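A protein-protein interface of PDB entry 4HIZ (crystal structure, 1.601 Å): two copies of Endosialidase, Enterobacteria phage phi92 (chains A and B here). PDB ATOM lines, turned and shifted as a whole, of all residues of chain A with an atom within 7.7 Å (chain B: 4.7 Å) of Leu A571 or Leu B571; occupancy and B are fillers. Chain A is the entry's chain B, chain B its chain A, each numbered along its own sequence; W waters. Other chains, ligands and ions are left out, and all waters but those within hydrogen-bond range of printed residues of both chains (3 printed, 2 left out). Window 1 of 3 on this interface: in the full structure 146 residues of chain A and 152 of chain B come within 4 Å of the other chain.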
ATOM      1  N   ASN A 564      23.163   4.370  35.297  1.00  0.00           N
ATOM      2  CA  ASN A 564      24.249   3.392  35.262  1.00  0.00           C
ATOM      3  C   ASN A 564      23.915   2.139  34.453  1.00  0.00           C
ATOM      4  O   ASN A 564      22.764   1.979  33.992  1.00  0.00           O
ATOM      5  CB  ASN A 564      24.593   2.999  36.695  1.00  0.00           C
ATOM      6  CG  ASN A 564      25.210   4.174  37.456  1.00  0.00           C
ATOM      7  OD1 ASN A 564      26.450   4.424  37.373  1.00  0.00           O
ATOM      8  ND2 ASN A 564      24.398   4.881  38.187  1.00  0.00           N
ATOM      9  N   ASP A 565      24.901   1.243  34.310  1.00  0.00           N
ATOM     10  CA  ASP A 565      24.685  -0.040  33.613  1.00  0.00           C
ATOM     11  C   ASP A 565      23.513  -0.825  34.190  1.00  0.00           C
ATOM     12  O   ASP A 565      23.401  -0.995  35.413  1.00  0.00           O
ATOM     13  CB  ASP A 565      25.928  -0.939  33.734  1.00  0.00           C
ATOM     14  CG  ASP A 565      27.140  -0.374  33.016  1.00  0.00           C
ATOM     15  OD1 ASP A 565      27.020   0.176  31.887  1.00  0.00           O
ATOM     16  OD2 ASP A 565      28.225  -0.467  33.605  1.00  0.00           O
ATOM     17  N   VAL A 566      22.669  -1.339  33.300  1.00  0.00           N
ATOM     18  CA  VAL A 566      21.551  -2.192  33.717  1.00  0.00           C
ATOM     19  C   VAL A 566      21.689  -3.574  33.065  1.00  0.00           C
ATOM     20  O   VAL A 566      22.048  -3.690  31.876  1.00  0.00           O
ATOM     21  CB  VAL A 566      20.213  -1.569  33.279  1.00  0.00           C
ATOM     22  CG1 VAL A 566      19.047  -2.545  33.599  1.00  0.00           C
ATOM     23  CG2 VAL A 566      19.994  -0.243  34.018  1.00  0.00           C
ATOM     24  N   GLN A 567      21.426  -4.620  33.846  1.00  0.00           N
ATOM     25  CA  GLN A 567      21.302  -5.975  33.272  1.00  0.00           C
ATOM     26  C   GLN A 567      19.939  -6.503  33.604  1.00  0.00           C
ATOM     27  O   GLN A 567      19.390  -6.163  34.650  1.00  0.00           O
ATOM     28  CB  GLN A 567      22.318  -6.941  33.897  1.00  0.00           C
ATOM     29  CG  GLN A 567      23.750  -6.455  33.765  1.00  0.00           C
ATOM     30  CD  GLN A 567      24.633  -7.614  33.993  1.00  0.00           C
ATOM     31  OE1 GLN A 567      25.319  -8.036  33.104  1.00  0.00           O
ATOM     32  NE2 GLN A 567      24.567  -8.183  35.181  1.00  0.00           N
ATOM     33  N   MET A 568      19.394  -7.366  32.749  1.00  0.00           N
ATOM     34  CA  MET A 568      18.121  -7.990  33.078  1.00  0.00           C
ATOM     35  C   MET A 568      18.047  -9.366  32.465  1.00  0.00           C
ATOM     36  O   MET A 568      18.671  -9.654  31.444  1.00  0.00           O
ATOM     37  CB  MET A 568      16.938  -7.135  32.610  1.00  0.00           C
ATOM     38  CG  MET A 568      16.959  -6.871  31.127  1.00  0.00           C
ATOM     39  SD  MET A 568      15.718  -5.651  30.668  1.00  0.00           S
ATOM     40  CE  MET A 568      16.320  -4.161  31.469  1.00  0.00           C
ATOM     41  N   TYR A 569      17.252 -10.211  33.098  1.00  0.00           N
ATOM     42  CA  TYR A 569      17.129 -11.599  32.661  1.00  0.00           C
ATOM     43  C   TYR A 569      16.617 -11.740  31.227  1.00  0.00           C
ATOM     44  O   TYR A 569      17.198 -12.474  30.419  1.00  0.00           O
ATOM     45  CB  TYR A 569      16.215 -12.361  33.625  1.00  0.00           C
ATOM     46  CG  TYR A 569      16.017 -13.807  33.225  1.00  0.00           C
ATOM     47  CD1 TYR A 569      16.978 -14.778  33.551  1.00  0.00           C
ATOM     48  CD2 TYR A 569      14.869 -14.198  32.524  1.00  0.00           C
ATOM     49  CE1 TYR A 569      16.814 -16.064  33.179  1.00  0.00           C
ATOM     50  CE2 TYR A 569      14.695 -15.521  32.161  1.00  0.00           C
ATOM     51  CZ  TYR A 569      15.686 -16.438  32.493  1.00  0.00           C
ATOM     52  OH  TYR A 569      15.555 -17.773  32.166  1.00  0.00           O
ATOM     53  N   SER A 570      15.521 -11.032  30.924  1.00  0.00           N
ATOM     54  CA  SER A 570      14.931 -10.991  29.591  1.00  0.00           C
ATOM     55  C   SER A 570      14.261  -9.631  29.502  1.00  0.00           C
ATOM     56  O   SER A 570      14.040  -8.954  30.521  1.00  0.00           O
ATOM     57  CB  SER A 570      13.886 -12.096  29.421  1.00  0.00           C
ATOM     58  OG  SER A 570      12.765 -11.844  30.254  1.00  0.00           O
ATOM     59  N   LEU A 571      13.947  -9.244  28.283  1.00  0.00           N
ATOM     60  CA  LEU A 571      13.301  -7.939  28.039  1.00  0.00           C
ATOM     61  C   LEU A 571      12.146  -8.092  27.045  1.00  0.00           C
ATOM     62  O   LEU A 571      12.322  -8.662  25.964  1.00  0.00           O
ATOM     63  CB  LEU A 571      14.338  -6.937  27.510  1.00  0.00           C
ATOM     64  CG  LEU A 571      13.710  -5.615  27.046  1.00  0.00           C
ATOM     65  CD1 LEU A 571      12.997  -4.883  28.205  1.00  0.00           C
ATOM     66  CD2 LEU A 571      14.822  -4.729  26.403  1.00  0.00           C
ATOM     67  N   THR A 572      10.980  -7.569  27.416  1.00  0.00           N
ATOM     68  CA  THR A 572       9.898  -7.356  26.436  1.00  0.00           C
ATOM     69  C   THR A 572       9.557  -5.876  26.425  1.00  0.00           C
ATOM     70  O   THR A 572       9.313  -5.281  27.485  1.00  0.00           O
ATOM     71  CB  THR A 572       8.627  -8.174  26.765  1.00  0.00           C
ATOM     72  OG1 THR A 572       8.993  -9.559  26.787  1.00  0.00           O
ATOM     73  CG2 THR A 572       7.515  -7.932  25.711  1.00  0.00           C
ATOM     74  N   VAL A 573       9.569  -5.284  25.239  1.00  0.00           N
ATOM     75  CA  VAL A 573       9.174  -3.867  25.121  1.00  0.00           C
ATOM     76  C   VAL A 573       7.712  -3.904  24.657  1.00  0.00           C
ATOM     77  O   VAL A 573       7.399  -4.535  23.641  1.00  0.00           O
ATOM     78  CB  VAL A 573      10.075  -3.111  24.148  1.00  0.00           C
ATOM     79  CG1 VAL A 573       9.779  -1.588  24.211  1.00  0.00           C
ATOM     80  CG2 VAL A 573      11.571  -3.332  24.513  1.00  0.00           C
ATOM     81  N   THR A 574       6.834  -3.257  25.429  1.00  0.00           N
ATOM     82  CA  THR A 574       5.389  -3.539  25.320  1.00  0.00           C
ATOM     83  C   THR A 574       4.561  -2.520  24.524  1.00  0.00           C
ATOM     84  O   THR A 574       3.599  -2.921  23.871  1.00  0.00           O
ATOM     85  CB  THR A 574       4.736  -3.601  26.734  1.00  0.00           C
ATOM     86  OG1 THR A 574       4.828  -2.301  27.355  1.00  0.00           O
ATOM     87  CG2 THR A 574       5.415  -4.666  27.618  1.00  0.00           C
ATOM     88  N   VAL A 588      12.612   0.897  20.487  1.00  0.00           N
ATOM     89  CA  VAL A 588      13.880   0.880  21.227  1.00  0.00           C
ATOM     90  C   VAL A 588      14.766   1.864  20.461  1.00  0.00           C
ATOM     91  O   VAL A 588      14.928   1.733  19.253  1.00  0.00           O
ATOM     92  CB  VAL A 588      14.536  -0.520  21.228  1.00  0.00           C
ATOM     93  CG1 VAL A 588      15.943  -0.451  21.846  1.00  0.00           C
ATOM     94  CG2 VAL A 588      13.639  -1.511  21.986  1.00  0.00           C
ATOM     95  N   VAL A 596      25.296   0.080  19.133  1.00  0.00           N
ATOM     96  CA  VAL A 596      25.833  -1.241  18.965  1.00  0.00           C
ATOM     97  C   VAL A 596      24.861  -2.243  19.623  1.00  0.00           C
ATOM     98  O   VAL A 596      24.537  -2.103  20.812  1.00  0.00           O
ATOM     99  CB  VAL A 596      27.210  -1.323  19.692  1.00  0.00           C
ATOM    100  CG1 VAL A 596      27.750  -2.764  19.662  1.00  0.00           C
ATOM    101  CG2 VAL A 596      28.225  -0.321  19.100  1.00  0.00           C
ATOM    102  N   ALA A 598      24.937  -6.201  20.202  1.00  0.00           N
ATOM    103  CA  ALA A 598      25.992  -7.189  20.012  1.00  0.00           C
ATOM    104  C   ALA A 598      25.762  -8.450  20.835  1.00  0.00           C
ATOM    105  O   ALA A 598      24.968  -8.464  21.807  1.00  0.00           O
ATOM    106  CB  ALA A 598      27.379  -6.592  20.400  1.00  0.00           C
ATOM    107  N   ASN A 600      27.524 -11.077  23.265  1.00  0.00           N
ATOM    108  CA  ASN A 600      28.657 -11.442  24.121  1.00  0.00           C
ATOM    109  C   ASN A 600      29.167 -12.845  23.829  1.00  0.00           C
ATOM    110  O   ASN A 600      28.450 -13.709  23.327  1.00  0.00           O
ATOM    111  CB  ASN A 600      28.277 -11.308  25.595  1.00  0.00           C
ATOM    112  CG  ASN A 600      28.239  -9.856  26.071  1.00  0.00           C
ATOM    113  OD1 ASN A 600      28.815  -8.974  25.455  1.00  0.00           O
ATOM    114  ND2 ASN A 600      27.579  -9.618  27.189  1.00  0.00           N
ATOM    115  N   MET B 568      18.106   3.999  29.901  1.00  0.00           N
ATOM    116  CA  MET B 568      19.195   3.430  30.693  1.00  0.00           C
ATOM    117  C   MET B 568      20.540   3.639  30.020  1.00  0.00           C
ATOM    118  O   MET B 568      20.653   3.758  28.796  1.00  0.00           O
ATOM    119  CB  MET B 568      18.979   1.949  30.965  1.00  0.00           C
ATOM    120  CG  MET B 568      18.914   1.157  29.710  1.00  0.00           C
ATOM    121  SD  MET B 568      18.435  -0.521  30.077  1.00  0.00           S
ATOM    122  CE  MET B 568      16.729  -0.371  30.644  1.00  0.00           C
ATOM    123  N   SER B 570      23.272   1.736  29.674  1.00  0.00           N
ATOM    124  CA  SER B 570      23.636   0.609  28.803  1.00  0.00           C
ATOM    125  C   SER B 570      22.723  -0.543  29.208  1.00  0.00           C
ATOM    126  O   SER B 570      22.105  -0.506  30.274  1.00  0.00           O
ATOM    127  CB  SER B 570      25.098   0.161  28.992  1.00  0.00           C
ATOM    128  OG  SER B 570      25.256  -0.430  30.273  1.00  0.00           O
ATOM    129  N   LEU B 571      22.676  -1.573  28.368  1.00  0.00           N
ATOM    130  CA  LEU B 571      21.806  -2.713  28.648  1.00  0.00           C
ATOM    131  C   LEU B 571      22.501  -4.012  28.291  1.00  0.00           C
ATOM    132  O   LEU B 571      23.079  -4.136  27.195  1.00  0.00           O
ATOM    133  CB  LEU B 571      20.515  -2.591  27.799  1.00  0.00           C
ATOM    134  CG  LEU B 571      19.618  -3.848  27.866  1.00  0.00           C
ATOM    135  CD1 LEU B 571      19.150  -4.155  29.290  1.00  0.00           C
ATOM    136  CD2 LEU B 571      18.396  -3.730  26.936  1.00  0.00           C
ATOM    137  N   THR B 572      22.462  -4.958  29.223  1.00  0.00           N
ATOM    138  CA  THR B 572      22.892  -6.334  28.937  1.00  0.00           C
ATOM    139  C   THR B 572      21.737  -7.238  29.299  1.00  0.00           C
ATOM    140  O   THR B 572      21.191  -7.130  30.392  1.00  0.00           O
ATOM    141  CB  THR B 572      24.147  -6.733  29.735  1.00  0.00           C
ATOM    142  OG1 THR B 572      25.223  -5.893  29.318  1.00  0.00           O
ATOM    143  CG2 THR B 572      24.532  -8.213  29.472  1.00  0.00           C
ATOM    144  N   VAL B 573      21.352  -8.112  28.378  1.00  0.00           N
ATOM    145  CA  VAL B 573      20.260  -9.057  28.669  1.00  0.00           C
ATOM    146  C   VAL B 573      20.977 -10.387  28.948  1.00  0.00           C
ATOM    147  O   VAL B 573      21.739 -10.851  28.110  1.00  0.00           O
ATOM    148  CB  VAL B 573      19.267  -9.160  27.498  1.00  0.00           C
ATOM    149  CG1 VAL B 573      18.017  -9.965  27.947  1.00  0.00           C
ATOM    150  CG2 VAL B 573      18.872  -7.734  27.046  1.00  0.00           C
ATOM    151  N   ARG B 587      16.715 -13.504  25.192  1.00  0.00           N
ATOM    152  CA  ARG B 587      15.641 -12.950  24.354  1.00  0.00           C
ATOM    153  C   ARG B 587      15.251 -11.503  24.650  1.00  0.00           C
ATOM    154  O   ARG B 587      14.999 -11.133  25.808  1.00  0.00           O
ATOM    155  CB  ARG B 587      14.378 -13.792  24.561  1.00  0.00           C
ATOM    156  CG  ARG B 587      14.586 -15.274  24.276  1.00  0.00           C
ATOM    157  CD  ARG B 587      13.372 -16.106  24.653  1.00  0.00           C
ATOM    158  NE  ARG B 587      13.453 -17.418  24.031  1.00  0.00           N
ATOM    159  CZ  ARG B 587      13.926 -18.511  24.609  1.00  0.00           C
ATOM    160  NH1 ARG B 587      14.395 -18.467  25.853  1.00  0.00           N
ATOM    161  NH2 ARG B 587      13.927 -19.656  23.925  1.00  0.00           N
ATOM    162  N   VAL B 588      15.132 -10.716  23.591  1.00  0.00           N
ATOM    163  CA  VAL B 588      14.484  -9.410  23.645  1.00  0.00           C
ATOM    164  C   VAL B 588      13.306  -9.518  22.688  1.00  0.00           C
ATOM    165  O   VAL B 588      13.492  -9.896  21.545  1.00  0.00           O
ATOM    166  CB  VAL B 588      15.423  -8.296  23.129  1.00  0.00           C
ATOM    167  CG1 VAL B 588      14.656  -6.956  23.025  1.00  0.00           C
ATOM    168  CG2 VAL B 588      16.622  -8.170  24.080  1.00  0.00           C
ATOM    169  N   LYS B 589      12.101  -9.234  23.158  1.00  0.00           N
ATOM    170  CA  LYS B 589      10.928  -9.322  22.275  1.00  0.00           C
ATOM    171  C   LYS B 589      10.207  -7.991  22.254  1.00  0.00           C
ATOM    172  O   LYS B 589      10.170  -7.283  23.256  1.00  0.00           O
ATOM    173  CB  LYS B 589       9.945 -10.397  22.767  1.00  0.00           C
ATOM    174  CG  LYS B 589      10.595 -11.760  22.938  1.00  0.00           C
ATOM    175  CD  LYS B 589       9.662 -12.679  23.720  1.00  0.00           C
ATOM    176  CE  LYS B 589      10.282 -14.037  23.975  1.00  0.00           C
ATOM    177  NZ  LYS B 589       9.310 -14.934  24.674  1.00  0.00           N
HETATM  178  O   HOH W   1      28.689   0.037  30.039  1.00  0.00           O
HETATM  179  O   HOH W   2      27.691  -7.076  28.812  1.00  0.00           O
HETATM  180  O   HOH W   3      24.753  -3.224  30.923  1.00  0.00           O
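The side-chain carboxylate of Asp A565 lies within hydrogen-bond range of the side-chain hydroxyl of Ser B570, at 2.5 Å. The backbone carbonyl oxygen of Ser B570 sits at hydrogen-bond distance from the backbone NH of Val A566 (3.2 Å). The backbone carbonyl oxygen of Val A566 lies within hydrogen-bond range of the backbone NH of Thr B572 (3.0 Å). The backbone carbonyl oxygen (O) of Thr B572 lies within hydrogen-bond range of the backbone NH (N) of Met A568 (3.0 Å). The backbone NH (N) of Leu A571 is in hydrogen-bond range of the backbone carbonyl oxygen (O) of Arg B587, 3.3 Å away. N of Lys B589 is in hydrogen-bond range of O of Leu A571. O of Lys B589 sits at hydrogen-bond distance from N of Val A573.
Leu B571 touches Val A566. Met A568 touches Met B568 (CE to CE, 3.9 Å). CE of Met A568 touches CD1 of Leu B571, at 3.6 Å. Met A568 touches Val B573 (O to CA, 3.3 Å). Tyr A569 touches Val B573. CA of Ser A570 touches CG1 of Val B573, 3.6 Å away. Ser A570 touches Arg B587 (CA to O, 3.8 Å). Leu B571 touches Leu A571. Val B588 touches Leu A571. O of Lys B589 touches CA of Thr A572, at 3.2 Å.
Printed residues of chain B within 4 Å of Met A568: Met B568 (3.9 Å), Leu B571 (3.6 Å), Thr B572 (3.0 Å) and Val B573 (3.3 Å). Printed residues of chain B within 4 Å of Ser A570: Val B573 (3.6 Å) and Arg B587 (3.8 Å). Of the printed residues of chain B, Leu A571 touches Leu B571 (3.7 Å), Arg B587 (3.3 Å), Val B588 (3.3 Å) and Lys B589 (2.9 Å). Val A588 touches none of the printed residues of chain B. Asn A600 touches none of the printed residues of chain B. Ser B570 touches just these residues of chain A: Asp A565 and Val A566. Of the printed residues of chain A, Leu B571 touches Val A566 (3.4 Å), Met A568 (3.6 Å) and Leu A571 (3.7 Å). The nearest printed residue of chain B that does not touch Leu A571 is Val B573 (4.1 Å). The nearest printed residue of chain A that does not touch Leu B571 is Gln A567 (4.9 Å). The nearest printed residue of chain A that does not touch Val B588 is Val A573 (5.0 Å).
Of the 8 printed residues of chain B, 8 touch a printed residue of chain A. Printed residues of chain B that touch a printed residue of chain A: Met B568, Ser B570, Leu B571, Thr B572, Val B573, Arg B587, Val B588 and Lys B589. Hydrophobic or aromatic side chains of chain B that line the printed part of chain A: Met B568, Leu B571 and Val B573. Hydrophobic or aromatic side chains of chain A within 4 Å of the printed part of chain B: Val A566, Met A568 and Leu A571. Among the printed residues, 19 pairs touch across the chains. Among the printed residues, no Asp or Glu carboxylate lies within 4 Å of a Lys or Arg side-chain nitrogen of the other chain.
Met A568 touches Thr B572, but with the chains exchanged Thr A572 does not touch Met B568 (9.4 Å). Met A568 touches Val B573, but with the chains exchanged Val A573 does not touch Met B568 (8.5 Å). Ser A570 touches Val B573, but with the chains exchanged Val A573 does not touch Ser B570 (12.3 Å). Leu A571 touches Val B588, but with the chains exchanged Val A588 does not touch Leu B571 (6.5 Å). Positions printed for both chains: 568, 570, 571, 572, 573 and 588.
Water W1 bridges OD1 of Asp A565 (2.5 Å) and OG of Ser B570 (3.5 Å). Water W2 bridges OG1 of Thr B572 (2.8 Å) and ND2 of Asn A600 (3.0 Å). Water W3 lies within hydrogen-bond range of O of Val A566 (2.9 Å), OG of Ser B570 (2.9 Å) and OG1 of Thr B572 (3.1 Å).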
